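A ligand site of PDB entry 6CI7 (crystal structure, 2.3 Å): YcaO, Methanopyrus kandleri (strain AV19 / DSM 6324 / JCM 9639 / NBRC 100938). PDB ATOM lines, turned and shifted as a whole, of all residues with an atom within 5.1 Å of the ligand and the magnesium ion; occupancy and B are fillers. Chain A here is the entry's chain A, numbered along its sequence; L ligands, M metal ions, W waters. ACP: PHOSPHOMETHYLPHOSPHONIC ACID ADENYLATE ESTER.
Water W1 lies within hydrogen-bond range of OE1 of Glu 81 (2.7 Å), OE1 of Glu 78 (3.0 Å) and O2B of the ligand (3.1 Å). Water W2 lies within hydrogen-bond range of the side-chain carboxylate of Glu 156 (2.9 Å) and a nitrogen (N1) of the ligand (2.9 Å). Water W4 bridges NH2 of Arg 12 and O1A of the ligand. Water W11 lies within hydrogen-bond range of the side-chain carboxylate (OE2) of Glu 251 (2.7 Å), an oxygen (O3G) of the ligand (3.3 Å) and the guanidinium group (NH2) of Arg 168 (3.3 Å). Water W3 lies within hydrogen-bond range of the side-chain hydroxyl (OG1) of Thr 19 and a nitrogen (N6) of the ligand. Water W5 lies within hydrogen-bond range of the guanidinium group of Arg 12 (2.9 Å) and a nitrogen (N7) of the ligand (3.3 Å).
O1G of the ligand binds the magnesium ion, at 1.9 Å. Water W6 is bound to the magnesium ion (2.1 Å). Water W1 is bound to the magnesium ion, at 2.1 Å. The magnesium ion is bound by water W10 (2.2 Å). The magnesium ion is bound by O1B of the ligand, at 2.3 Å. The magnesium ion is bound by OE2 of Glu 164, at 2.3 Å.
OE2 of Glu 81 touches the magnesium ion, at 3.8 Å. O of Leu 148 touches the magnesium ion, at 3.8 Å. Of the 26 residues printed, 3 come within 4 Å of the magnesium ion. Along chain A the residues within 4 Å of the magnesium ion span positions 81 to 164. The nearest printed residue that does not touch the magnesium ion is Gln 160 (4.4 Å).
OE1 of Glu 81 lies within hydrogen-bond range of O3' of the ligand, 2.5 Å away. An oxygen (O3G) of the ligand is in salt-bridge range of the guanidinium group (NH2) of Arg 168 (2.8 Å). An oxygen (O3') of the ligand is in hydrogen-bond range of the backbone NH of Ala 150, 3.1 Å away. An oxygen (O2') of the ligand sits at hydrogen-bond distance from the backbone carbonyl oxygen of Ala 150, 2.8 Å away. The guanidinium group (NH2) of Arg 12 sits at hydrogen-bond distance from an oxygen (O2') of the ligand (2.8 Å). The side-chain amide nitrogen of Gln 160 lies close to an oxygen (O1B) of the ligand, 2.9 Å away. An oxygen (O1A) of the ligand lies within salt-bridge range of the guanidinium group of Arg 247. The side-chain amide nitrogen (NE2) of Gln 70 lies within hydrogen-bond range of a nitrogen (N7) of the ligand (3.0 Å). The side-chain hydroxyl (OG) of Ser 74 is in hydrogen-bond range of an oxygen (O2A) of the ligand (3.0 Å). O2B of the ligand sits close to OE1 of Glu 78 (3.1 Å). The side-chain amino group of Lys 64 is in salt-bridge range of an oxygen (O2A) of the ligand (3.3 Å). The side-chain hydroxyl (OG) of Ser 149 lies within hydrogen-bond range of an oxygen (O2') of the ligand, at 3.4 Å.
Residues that only touch the ligand: Met 77, Glu 251, Val 73, Thr 19, Glu 156 and Gly 151. Hydrophobic or aromatic side chains that line the ligand: Val 73 and Met 77. The nearest printed residue that does not touch the ligand is Val 267 (4.1 Å).
The guanidinium group of Arg 82 lies within salt-bridge range of the side-chain carboxylate of Glu 81, 2.8 Å away. The guanidinium group (NH1) of Arg 12 lies within salt-bridge range of the side-chain carboxylate (OE2) of Glu 156 (3.2 Å). NE2 of Gln 160 sits close to NH2 of Arg 247, 3.2 Å away. The side-chain amide oxygen of Gln 160 sits at hydrogen-bond distance from the side-chain hydroxyl of Ser 149. The backbone carbonyl oxygen (O) of Glu 9 is in hydrogen-bond range of the guanidinium group (NH1) of Arg 247 (3.1 Å). The side-chain hydroxyl of Ser 74 is in hydrogen-bond range of the backbone NH of Lys 64, at 3.0 Å. The side-chain hydroxyl of Thr 19 sits at hydrogen-bond distance from the guanidinium group of Arg 152 (2.9 Å). The side-chain carboxylate of Glu 156 sits at hydrogen-bond distance from the backbone NH of Arg 152.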
ATOM      1  N   GLU A   9      19.036 -34.054  14.758  1.00  0.00           N
ATOM      2  CA  GLU A   9      18.770 -33.030  13.720  1.00  0.00           C
ATOM      3  C   GLU A   9      20.046 -32.467  13.112  1.00  0.00           C
ATOM      4  O   GLU A   9      20.004 -31.829  12.077  1.00  0.00           O
ATOM      5  CB  GLU A   9      17.941 -31.863  14.283  1.00  0.00           C
ATOM      6  CG  GLU A   9      16.501 -32.203  14.621  1.00  0.00           C
ATOM      7  CD  GLU A   9      16.318 -32.775  16.018  1.00  0.00           C
ATOM      8  OE1 GLU A   9      17.317 -32.913  16.767  1.00  0.00           O
ATOM      9  OE2 GLU A   9      15.170 -33.069  16.380  1.00  0.00           O
ATOM     10  N   ARG A  12      26.112 -32.049  17.228  1.00  0.00           N
ATOM     11  CA  ARG A  12      26.237 -31.080  18.333  1.00  0.00           C
ATOM     12  C   ARG A  12      27.134 -31.575  19.475  1.00  0.00           C
ATOM     13  O   ARG A  12      27.134 -32.761  19.807  1.00  0.00           O
ATOM     14  CB  ARG A  12      24.853 -30.647  18.879  1.00  0.00           C
ATOM     15  CG  ARG A  12      23.884 -30.081  17.824  1.00  0.00           C
ATOM     16  CD  ARG A  12      24.382 -28.760  17.208  1.00  0.00           C
ATOM     17  NE  ARG A  12      23.640 -28.394  16.007  1.00  0.00           N
ATOM     18  CZ  ARG A  12      23.751 -27.235  15.349  1.00  0.00           C
ATOM     19  NH1 ARG A  12      24.580 -26.277  15.756  1.00  0.00           N
ATOM     20  NH2 ARG A  12      23.020 -27.027  14.270  1.00  0.00           N
ATOM     21  N   PRO A  16      20.515 -30.652  23.511  1.00  0.00           N
ATOM     22  CA  PRO A  16      19.629 -29.499  23.359  1.00  0.00           C
ATOM     23  C   PRO A  16      19.096 -28.884  24.677  1.00  0.00           C
ATOM     24  O   PRO A  16      18.945 -27.662  24.742  1.00  0.00           O
ATOM     25  CB  PRO A  16      18.494 -30.034  22.468  1.00  0.00           C
ATOM     26  CG  PRO A  16      19.175 -31.066  21.633  1.00  0.00           C
ATOM     27  CD  PRO A  16      20.140 -31.740  22.578  1.00  0.00           C
ATOM     28  N   THR A  19      21.764 -26.518  25.862  1.00  0.00           N
ATOM     29  CA  THR A  19      21.808 -25.372  24.970  1.00  0.00           C
ATOM     30  C   THR A  19      20.629 -24.425  25.214  1.00  0.00           C
ATOM     31  O   THR A  19      20.840 -23.218  25.251  1.00  0.00           O
ATOM     32  CB  THR A  19      21.945 -25.823  23.514  1.00  0.00           C
ATOM     33  OG1 THR A  19      23.160 -26.577  23.410  1.00  0.00           O
ATOM     34  CG2 THR A  19      21.990 -24.629  22.531  1.00  0.00           C
ATOM     35  N   GLY A  63      11.614 -22.329  13.826  1.00  0.00           N
ATOM     36  CA  GLY A  63      12.418 -23.447  14.284  1.00  0.00           C
ATOM     37  C   GLY A  63      11.566 -24.695  14.406  1.00  0.00           C
ATOM     38  O   GLY A  63      10.342 -24.619  14.481  1.00  0.00           O
ATOM     39  N   LYS A  64      12.221 -25.854  14.430  1.00  0.00           N
ATOM     40  CA  LYS A  64      11.542 -27.139  14.508  1.00  0.00           C
ATOM     41  C   LYS A  64      12.533 -28.168  15.047  1.00  0.00           C
ATOM     42  O   LYS A  64      13.729 -27.858  15.167  1.00  0.00           O
ATOM     43  CB  LYS A  64      10.960 -27.551  13.136  1.00  0.00           C
ATOM     44  CG  LYS A  64      11.939 -28.124  12.117  1.00  0.00           C
ATOM     45  CD  LYS A  64      12.815 -27.055  11.481  1.00  0.00           C
ATOM     46  CE  LYS A  64      13.603 -27.620  10.306  1.00  0.00           C
ATOM     47  NZ  LYS A  64      14.304 -26.544   9.570  1.00  0.00           N
ATOM     48  N   GLN A  70      14.383 -28.973  21.297  1.00  0.00           N
ATOM     49  CA  GLN A  70      15.099 -28.755  20.047  1.00  0.00           C
ATOM     50  C   GLN A  70      14.445 -27.705  19.121  1.00  0.00           C
ATOM     51  O   GLN A  70      15.148 -26.852  18.584  1.00  0.00           O
ATOM     52  CB  GLN A  70      15.378 -30.082  19.300  1.00  0.00           C
ATOM     53  CG  GLN A  70      16.091 -29.939  17.942  1.00  0.00           C
ATOM     54  CD  GLN A  70      17.390 -29.147  17.978  1.00  0.00           C
ATOM     55  OE1 GLN A  70      18.093 -29.109  18.993  1.00  0.00           O
ATOM     56  NE2 GLN A  70      17.719 -28.504  16.859  1.00  0.00           N
ATOM     57  N   VAL A  73      15.342 -24.311  20.685  1.00  0.00           N
ATOM     58  CA  VAL A  73      16.743 -23.940  20.397  1.00  0.00           C
ATOM     59  C   VAL A  73      16.933 -23.575  18.930  1.00  0.00           C
ATOM     60  O   VAL A  73      17.494 -22.515  18.624  1.00  0.00           O
ATOM     61  CB  VAL A  73      17.862 -24.870  20.974  1.00  0.00           C
ATOM     62  CG1 VAL A  73      17.343 -26.027  21.821  1.00  0.00           C
ATOM     63  CG2 VAL A  73      18.933 -25.230  19.941  1.00  0.00           C
ATOM     64  N   SER A  74      16.450 -24.434  18.039  1.00  0.00           N
ATOM     65  CA  SER A  74      16.441 -24.166  16.597  1.00  0.00           C
ATOM     66  C   SER A  74      15.869 -22.745  16.249  1.00  0.00           C
ATOM     67  O   SER A  74      16.530 -21.978  15.531  1.00  0.00           O
ATOM     68  CB  SER A  74      15.717 -25.309  15.888  1.00  0.00           C
ATOM     69  OG  SER A  74      15.027 -24.893  14.738  1.00  0.00           O
ATOM     70  N   MET A  77      18.300 -19.906  17.772  1.00  0.00           N
ATOM     71  CA  MET A  77      19.583 -19.799  17.052  1.00  0.00           C
ATOM     72  C   MET A  77      19.403 -19.301  15.637  1.00  0.00           C
ATOM     73  O   MET A  77      20.269 -18.606  15.102  1.00  0.00           O
ATOM     74  CB  MET A  77      20.315 -21.128  17.134  1.00  0.00           C
ATOM     75  CG  MET A  77      20.608 -21.541  18.580  1.00  0.00           C
ATOM     76  SD  MET A  77      21.932 -20.307  19.351  1.00  0.00           S
ATOM     77  CE  MET A  77      23.525 -21.131  18.504  1.00  0.00           C
ATOM     78  N   GLU A  78      18.277 -19.633  15.014  1.00  0.00           N
ATOM     79  CA  GLU A  78      17.875 -19.041  13.743  1.00  0.00           C
ATOM     80  C   GLU A  78      17.789 -17.479  13.840  1.00  0.00           C
ATOM     81  O   GLU A  78      18.238 -16.772  12.922  1.00  0.00           O
ATOM     82  CB  GLU A  78      16.556 -19.672  13.281  1.00  0.00           C
ATOM     83  CG  GLU A  78      15.838 -19.012  12.124  1.00  0.00           C
ATOM     84  CD  GLU A  78      16.298 -19.495  10.767  1.00  0.00           C
ATOM     85  OE1 GLU A  78      16.445 -20.721  10.561  1.00  0.00           O
ATOM     86  OE2 GLU A  78      16.503 -18.643   9.895  1.00  0.00           O
ATOM     87  N   GLU A  81      21.507 -16.165  14.211  1.00  0.00           N
ATOM     88  CA  GLU A  81      22.253 -16.157  12.941  1.00  0.00           C
ATOM     89  C   GLU A  81      21.851 -14.973  12.077  1.00  0.00           C
ATOM     90  O   GLU A  81      22.724 -14.337  11.491  1.00  0.00           O
ATOM     91  CB  GLU A  81      22.179 -17.495  12.171  1.00  0.00           C
ATOM     92  CG  GLU A  81      20.981 -17.687  11.270  1.00  0.00           C
ATOM     93  CD  GLU A  81      21.049 -18.940  10.405  1.00  0.00           C
ATOM     94  OE1 GLU A  81      21.234 -20.041  10.959  1.00  0.00           O
ATOM     95  OE2 GLU A  81      20.871 -18.837   9.169  1.00  0.00           O
ATOM     96  N   ARG A  82      20.559 -14.651  12.039  1.00  0.00           N
ATOM     97  CA  ARG A  82      20.060 -13.540  11.222  1.00  0.00           C
ATOM     98  C   ARG A  82      20.542 -12.189  11.725  1.00  0.00           C
ATOM     99  O   ARG A  82      20.927 -11.336  10.924  1.00  0.00           O
ATOM    100  CB  ARG A  82      18.535 -13.556  11.117  1.00  0.00           C
ATOM    101  CG  ARG A  82      17.948 -14.679  10.282  1.00  0.00           C
ATOM    102  CD  ARG A  82      18.286 -14.543   8.809  1.00  0.00           C
ATOM    103  NE  ARG A  82      17.429 -15.380   7.959  1.00  0.00           N
ATOM    104  CZ  ARG A  82      17.608 -16.681   7.730  1.00  0.00           C
ATOM    105  NH1 ARG A  82      18.618 -17.366   8.272  1.00  0.00           N
ATOM    106  NH2 ARG A  82      16.750 -17.314   6.944  1.00  0.00           N
ATOM    107  N   LEU A 148      24.707 -19.705   5.846  1.00  0.00           N
ATOM    108  CA  LEU A 148      24.730 -19.017   7.112  1.00  0.00           C
ATOM    109  C   LEU A 148      24.342 -19.959   8.242  1.00  0.00           C
ATOM    110  O   LEU A 148      23.376 -20.703   8.124  1.00  0.00           O
ATOM    111  CB  LEU A 148      23.730 -17.883   7.008  1.00  0.00           C
ATOM    112  CG  LEU A 148      23.591 -16.778   8.017  1.00  0.00           C
ATOM    113  CD1 LEU A 148      24.883 -15.982   8.060  1.00  0.00           C
ATOM    114  CD2 LEU A 148      22.423 -15.940   7.564  1.00  0.00           C
ATOM    115  N   SER A 149      25.088 -19.947   9.335  1.00  0.00           N
ATOM    116  CA  SER A 149      24.820 -20.873  10.423  1.00  0.00           C
ATOM    117  C   SER A 149      25.383 -20.438  11.754  1.00  0.00           C
ATOM    118  O   SER A 149      26.486 -19.927  11.830  1.00  0.00           O
ATOM    119  CB  SER A 149      25.343 -22.279  10.064  1.00  0.00           C
ATOM    120  OG  SER A 149      25.090 -23.177  11.112  1.00  0.00           O
ATOM    121  N   ALA A 150      24.613 -20.688  12.805  1.00  0.00           N
ATOM    122  CA  ALA A 150      25.025 -20.457  14.193  1.00  0.00           C
ATOM    123  C   ALA A 150      25.232 -21.802  14.875  1.00  0.00           C
ATOM    124  O   ALA A 150      24.633 -22.796  14.475  1.00  0.00           O
ATOM    125  CB  ALA A 150      23.973 -19.641  14.943  1.00  0.00           C
ATOM    126  N   GLY A 151      26.099 -21.832  15.896  1.00  0.00           N
ATOM    127  CA  GLY A 151      26.258 -23.019  16.745  1.00  0.00           C
ATOM    128  C   GLY A 151      26.878 -22.684  18.101  1.00  0.00           C
ATOM    129  O   GLY A 151      27.214 -21.519  18.364  1.00  0.00           O
ATOM    130  N   ARG A 152      27.051 -23.684  18.949  1.00  0.00           N
ATOM    131  CA  ARG A 152      27.793 -23.493  20.209  1.00  0.00           C
ATOM    132  C   ARG A 152      29.313 -23.362  20.007  1.00  0.00           C
ATOM    133  O   ARG A 152      30.002 -22.669  20.773  1.00  0.00           O
ATOM    134  CB  ARG A 152      27.482 -24.599  21.215  1.00  0.00           C
ATOM    135  CG  ARG A 152      26.068 -24.572  21.791  1.00  0.00           C
ATOM    136  CD  ARG A 152      25.832 -23.483  22.820  1.00  0.00           C
ATOM    137  NE  ARG A 152      26.571 -23.621  24.085  1.00  0.00           N
ATOM    138  CZ  ARG A 152      26.237 -24.417  25.100  1.00  0.00           C
ATOM    139  NH1 ARG A 152      25.164 -25.196  25.044  1.00  0.00           N
ATOM    140  NH2 ARG A 152      26.992 -24.433  26.198  1.00  0.00           N
ATOM    141  N   GLU A 156      30.395 -26.605  14.741  1.00  0.00           N
ATOM    142  CA  GLU A 156      28.972 -26.901  14.543  1.00  0.00           C
ATOM    143  C   GLU A 156      28.419 -26.116  13.376  1.00  0.00           C
ATOM    144  O   GLU A 156      27.741 -26.686  12.508  1.00  0.00           O
ATOM    145  CB  GLU A 156      28.155 -26.596  15.780  1.00  0.00           C
ATOM    146  CG  GLU A 156      28.227 -27.652  16.859  1.00  0.00           C
ATOM    147  CD  GLU A 156      27.434 -27.245  18.086  1.00  0.00           C
ATOM    148  OE1 GLU A 156      27.384 -28.036  19.052  1.00  0.00           O
ATOM    149  OE2 GLU A 156      26.838 -26.141  18.067  1.00  0.00           O
ATOM    150  N   GLN A 160      27.095 -27.370   9.676  1.00  0.00           N
ATOM    151  CA  GLN A 160      25.711 -27.135   9.303  1.00  0.00           C
ATOM    152  C   GLN A 160      25.584 -26.249   8.071  1.00  0.00           C
ATOM    153  O   GLN A 160      24.805 -26.545   7.160  1.00  0.00           O
ATOM    154  CB  GLN A 160      24.942 -26.580  10.499  1.00  0.00           C
ATOM    155  CG  GLN A 160      23.461 -26.943  10.504  1.00  0.00           C
ATOM    156  CD  GLN A 160      22.617 -25.877   9.854  1.00  0.00           C
ATOM    157  OE1 GLN A 160      23.059 -24.744   9.663  1.00  0.00           O
ATOM    158  NE2 GLN A 160      21.376 -26.235   9.506  1.00  0.00           N
ATOM    159  N   GLU A 164      24.238 -27.201   4.231  1.00  0.00           N
ATOM    160  CA  GLU A 164      23.183 -26.375   3.644  1.00  0.00           C
ATOM    161  C   GLU A 164      23.540 -26.000   2.206  1.00  0.00           C
ATOM    162  O   GLU A 164      22.664 -26.061   1.317  1.00  0.00           O
ATOM    163  CB  GLU A 164      22.948 -25.133   4.522  1.00  0.00           C
ATOM    164  CG  GLU A 164      21.900 -24.165   4.017  1.00  0.00           C
ATOM    165  CD  GLU A 164      21.552 -23.118   5.066  1.00  0.00           C
ATOM    166  OE1 GLU A 164      21.900 -21.933   4.856  1.00  0.00           O
ATOM    167  OE2 GLU A 164      20.947 -23.482   6.114  1.00  0.00           O
ATOM    168  N   ARG A 168      21.528 -27.102  -1.223  1.00  0.00           N
ATOM    169  CA  ARG A 168      20.955 -26.196  -2.238  1.00  0.00           C
ATOM    170  C   ARG A 168      21.613 -26.376  -3.599  1.00  0.00           C
ATOM    171  O   ARG A 168      20.997 -26.107  -4.619  1.00  0.00           O
ATOM    172  CB  ARG A 168      20.940 -24.718  -1.790  1.00  0.00           C
ATOM    173  CG  ARG A 168      20.381 -24.491  -0.391  1.00  0.00           C
ATOM    174  CD  ARG A 168      18.888 -24.245  -0.319  1.00  0.00           C
ATOM    175  NE  ARG A 168      18.393 -24.371   1.055  1.00  0.00           N
ATOM    176  CZ  ARG A 168      18.556 -23.465   2.024  1.00  0.00           C
ATOM    177  NH1 ARG A 168      19.206 -22.319   1.814  1.00  0.00           N
ATOM    178  NH2 ARG A 168      18.069 -23.705   3.246  1.00  0.00           N
ATOM    179  N   ARG A 247      15.587 -34.253   8.457  1.00  0.00           N
ATOM    180  CA  ARG A 247      15.612 -32.820   8.190  1.00  0.00           C
ATOM    181  C   ARG A 247      14.664 -32.389   7.060  1.00  0.00           C
ATOM    182  O   ARG A 247      14.057 -31.305   7.126  1.00  0.00           O
ATOM    183  CB  ARG A 247      17.039 -32.373   7.932  1.00  0.00           C
ATOM    184  CG  ARG A 247      17.907 -32.422   9.186  1.00  0.00           C
ATOM    185  CD  ARG A 247      19.304 -31.869   8.939  1.00  0.00           C
ATOM    186  NE  ARG A 247      19.269 -30.466   8.493  1.00  0.00           N
ATOM    187  CZ  ARG A 247      18.991 -29.402   9.246  1.00  0.00           C
ATOM    188  NH1 ARG A 247      18.693 -29.520  10.536  1.00  0.00           N
ATOM    189  NH2 ARG A 247      18.993 -28.209   8.688  1.00  0.00           N
ATOM    190  N   GLU A 251      11.403 -30.086   7.769  1.00  0.00           N
ATOM    191  CA  GLU A 251      11.236 -28.873   6.970  1.00  0.00           C
ATOM    192  C   GLU A 251       9.849 -28.753   6.325  1.00  0.00           C
ATOM    193  O   GLU A 251       9.330 -27.652   6.151  1.00  0.00           O
ATOM    194  CB  GLU A 251      12.356 -28.746   5.931  1.00  0.00           C
ATOM    195  CG  GLU A 251      12.568 -27.319   5.480  1.00  0.00           C
ATOM    196  CD  GLU A 251      14.008 -27.040   5.211  1.00  0.00           C
ATOM    197  OE1 GLU A 251      14.431 -27.211   4.033  1.00  0.00           O
ATOM    198  OE2 GLU A 251      14.707 -26.656   6.194  1.00  0.00           O
ATOM    199  N   GLN A 254       7.633 -27.582   9.147  1.00  0.00           N
ATOM    200  CA  GLN A 254       7.876 -26.155   9.240  1.00  0.00           C
ATOM    201  C   GLN A 254       7.081 -25.388   8.164  1.00  0.00           C
ATOM    202  O   GLN A 254       6.373 -24.451   8.487  1.00  0.00           O
ATOM    203  CB  GLN A 254       9.369 -25.841   9.114  1.00  0.00           C
ATOM    204  CG  GLN A 254       9.743 -24.527   9.763  1.00  0.00           C
ATOM    205  CD  GLN A 254      11.107 -24.029   9.345  1.00  0.00           C
ATOM    206  OE1 GLN A 254      12.097 -24.241  10.035  1.00  0.00           O
ATOM    207  NE2 GLN A 254      11.155 -23.357   8.205  1.00  0.00           N
ATOM    208  N   VAL A 267      12.027 -18.471   3.206  1.00  0.00           N
ATOM    209  CA  VAL A 267      12.709 -19.311   4.216  1.00  0.00           C
ATOM    210  C   VAL A 267      12.070 -20.702   4.433  1.00  0.00           C
ATOM    211  O   VAL A 267      12.711 -21.618   4.952  1.00  0.00           O
ATOM    212  CB  VAL A 267      12.910 -18.564   5.583  1.00  0.00           C
ATOM    213  CG1 VAL A 267      13.756 -17.311   5.412  1.00  0.00           C
ATOM    214  CG2 VAL A 267      11.582 -18.222   6.261  1.00  0.00           C
HETATM  215  PG  ACP L   1      16.990 -23.122   6.733  1.00  0.00           P
HETATM  216  O1G ACP L   1      18.465 -22.488   6.574  1.00  0.00           O
HETATM  217  O2G ACP L   1      16.088 -22.143   7.637  1.00  0.00           O
HETATM  218  O3G ACP L   1      16.403 -23.236   5.391  1.00  0.00           O
HETATM  219  PB  ACP L   1      17.910 -24.705   9.038  1.00  0.00           P
HETATM  220  O1B ACP L   1      19.427 -24.326   8.623  1.00  0.00           O
HETATM  221  O2B ACP L   1      17.228 -23.553   9.678  1.00  0.00           O
HETATM  222  C3B ACP L   1      17.020 -24.806   7.468  1.00  0.00           C
HETATM  223  PA  ACP L   1      17.716 -25.815  11.727  1.00  0.00           P
HETATM  224  O1A ACP L   1      18.233 -27.078  12.377  1.00  0.00           O
HETATM  225  O2A ACP L   1      16.270 -25.488  12.029  1.00  0.00           O
HETATM  226  O3A ACP L   1      17.894 -25.952  10.096  1.00  0.00           O
HETATM  227  O5' ACP L   1      18.672 -24.657  12.268  1.00  0.00           O
HETATM  228  C5' ACP L   1      18.320 -23.324  12.682  1.00  0.00           C
HETATM  229  C4' ACP L   1      19.587 -22.598  13.182  1.00  0.00           C
HETATM  230  O4' ACP L   1      19.812 -22.971  14.551  1.00  0.00           O
HETATM  231  C3' ACP L   1      20.871 -23.005  12.453  1.00  0.00           C
HETATM  232  O3' ACP L   1      21.811 -21.924  12.468  1.00  0.00           O
HETATM  233  C2' ACP L   1      21.358 -24.167  13.297  1.00  0.00           C
HETATM  234  O2' ACP L   1      22.737 -24.428  13.159  1.00  0.00           O
HETATM  235  C1' ACP L   1      21.038 -23.694  14.696  1.00  0.00           C
HETATM  236  N9  ACP L   1      20.860 -24.835  15.609  1.00  0.00           N
HETATM  237  C8  ACP L   1      19.961 -25.809  15.456  1.00  0.00           C
HETATM  238  N7  ACP L   1      20.059 -26.728  16.440  1.00  0.00           N
HETATM  239  C5  ACP L   1      21.048 -26.327  17.263  1.00  0.00           C
HETATM  240  C6  ACP L   1      21.672 -26.835  18.509  1.00  0.00           C
HETATM  241  N6  ACP L   1      21.206 -27.978  19.074  1.00  0.00           N
HETATM  242  N1  ACP L   1      22.674 -26.124  19.050  1.00  0.00           N
HETATM  243  C2  ACP L   1      23.128 -24.974  18.485  1.00  0.00           C
HETATM  244  N3  ACP L   1      22.617 -24.452  17.346  1.00  0.00           N
HETATM  245  C4  ACP L   1      21.576 -25.070  16.701  1.00  0.00           C
HETATM  246 MG    MG M   1      19.940 -22.253   7.782  1.00  0.00          MG
HETATM  247  O   HOH W   1      19.249 -21.186   9.474  1.00  0.00           O
HETATM  248  O   HOH W   2      24.963 -27.278  20.481  1.00  0.00           O
HETATM  249  O   HOH W   3      22.988 -28.521  21.512  1.00  0.00           O
HETATM  250  O   HOH W   4      20.815 -28.359  13.126  1.00  0.00           O
HETATM  251  O   HOH W   5      21.087 -29.772  15.503  1.00  0.00           O
HETATM  252  O   HOH W   6      21.724 -22.613   8.768  1.00  0.00           O
HETATM  253  O   HOH W   7      19.908 -26.408   6.234  1.00  0.00           O
HETATM  254  O   HOH W   8      14.812 -23.243  11.101  1.00  0.00           O
HETATM  255  O   HOH W   9      16.338 -28.502  14.117  1.00  0.00           O
HETATM  256  O   HOH W  10      20.969 -20.433   7.084  1.00  0.00           O
HETATM  257  O   HOH W  11      17.091 -26.383   4.930  1.00  0.00           O
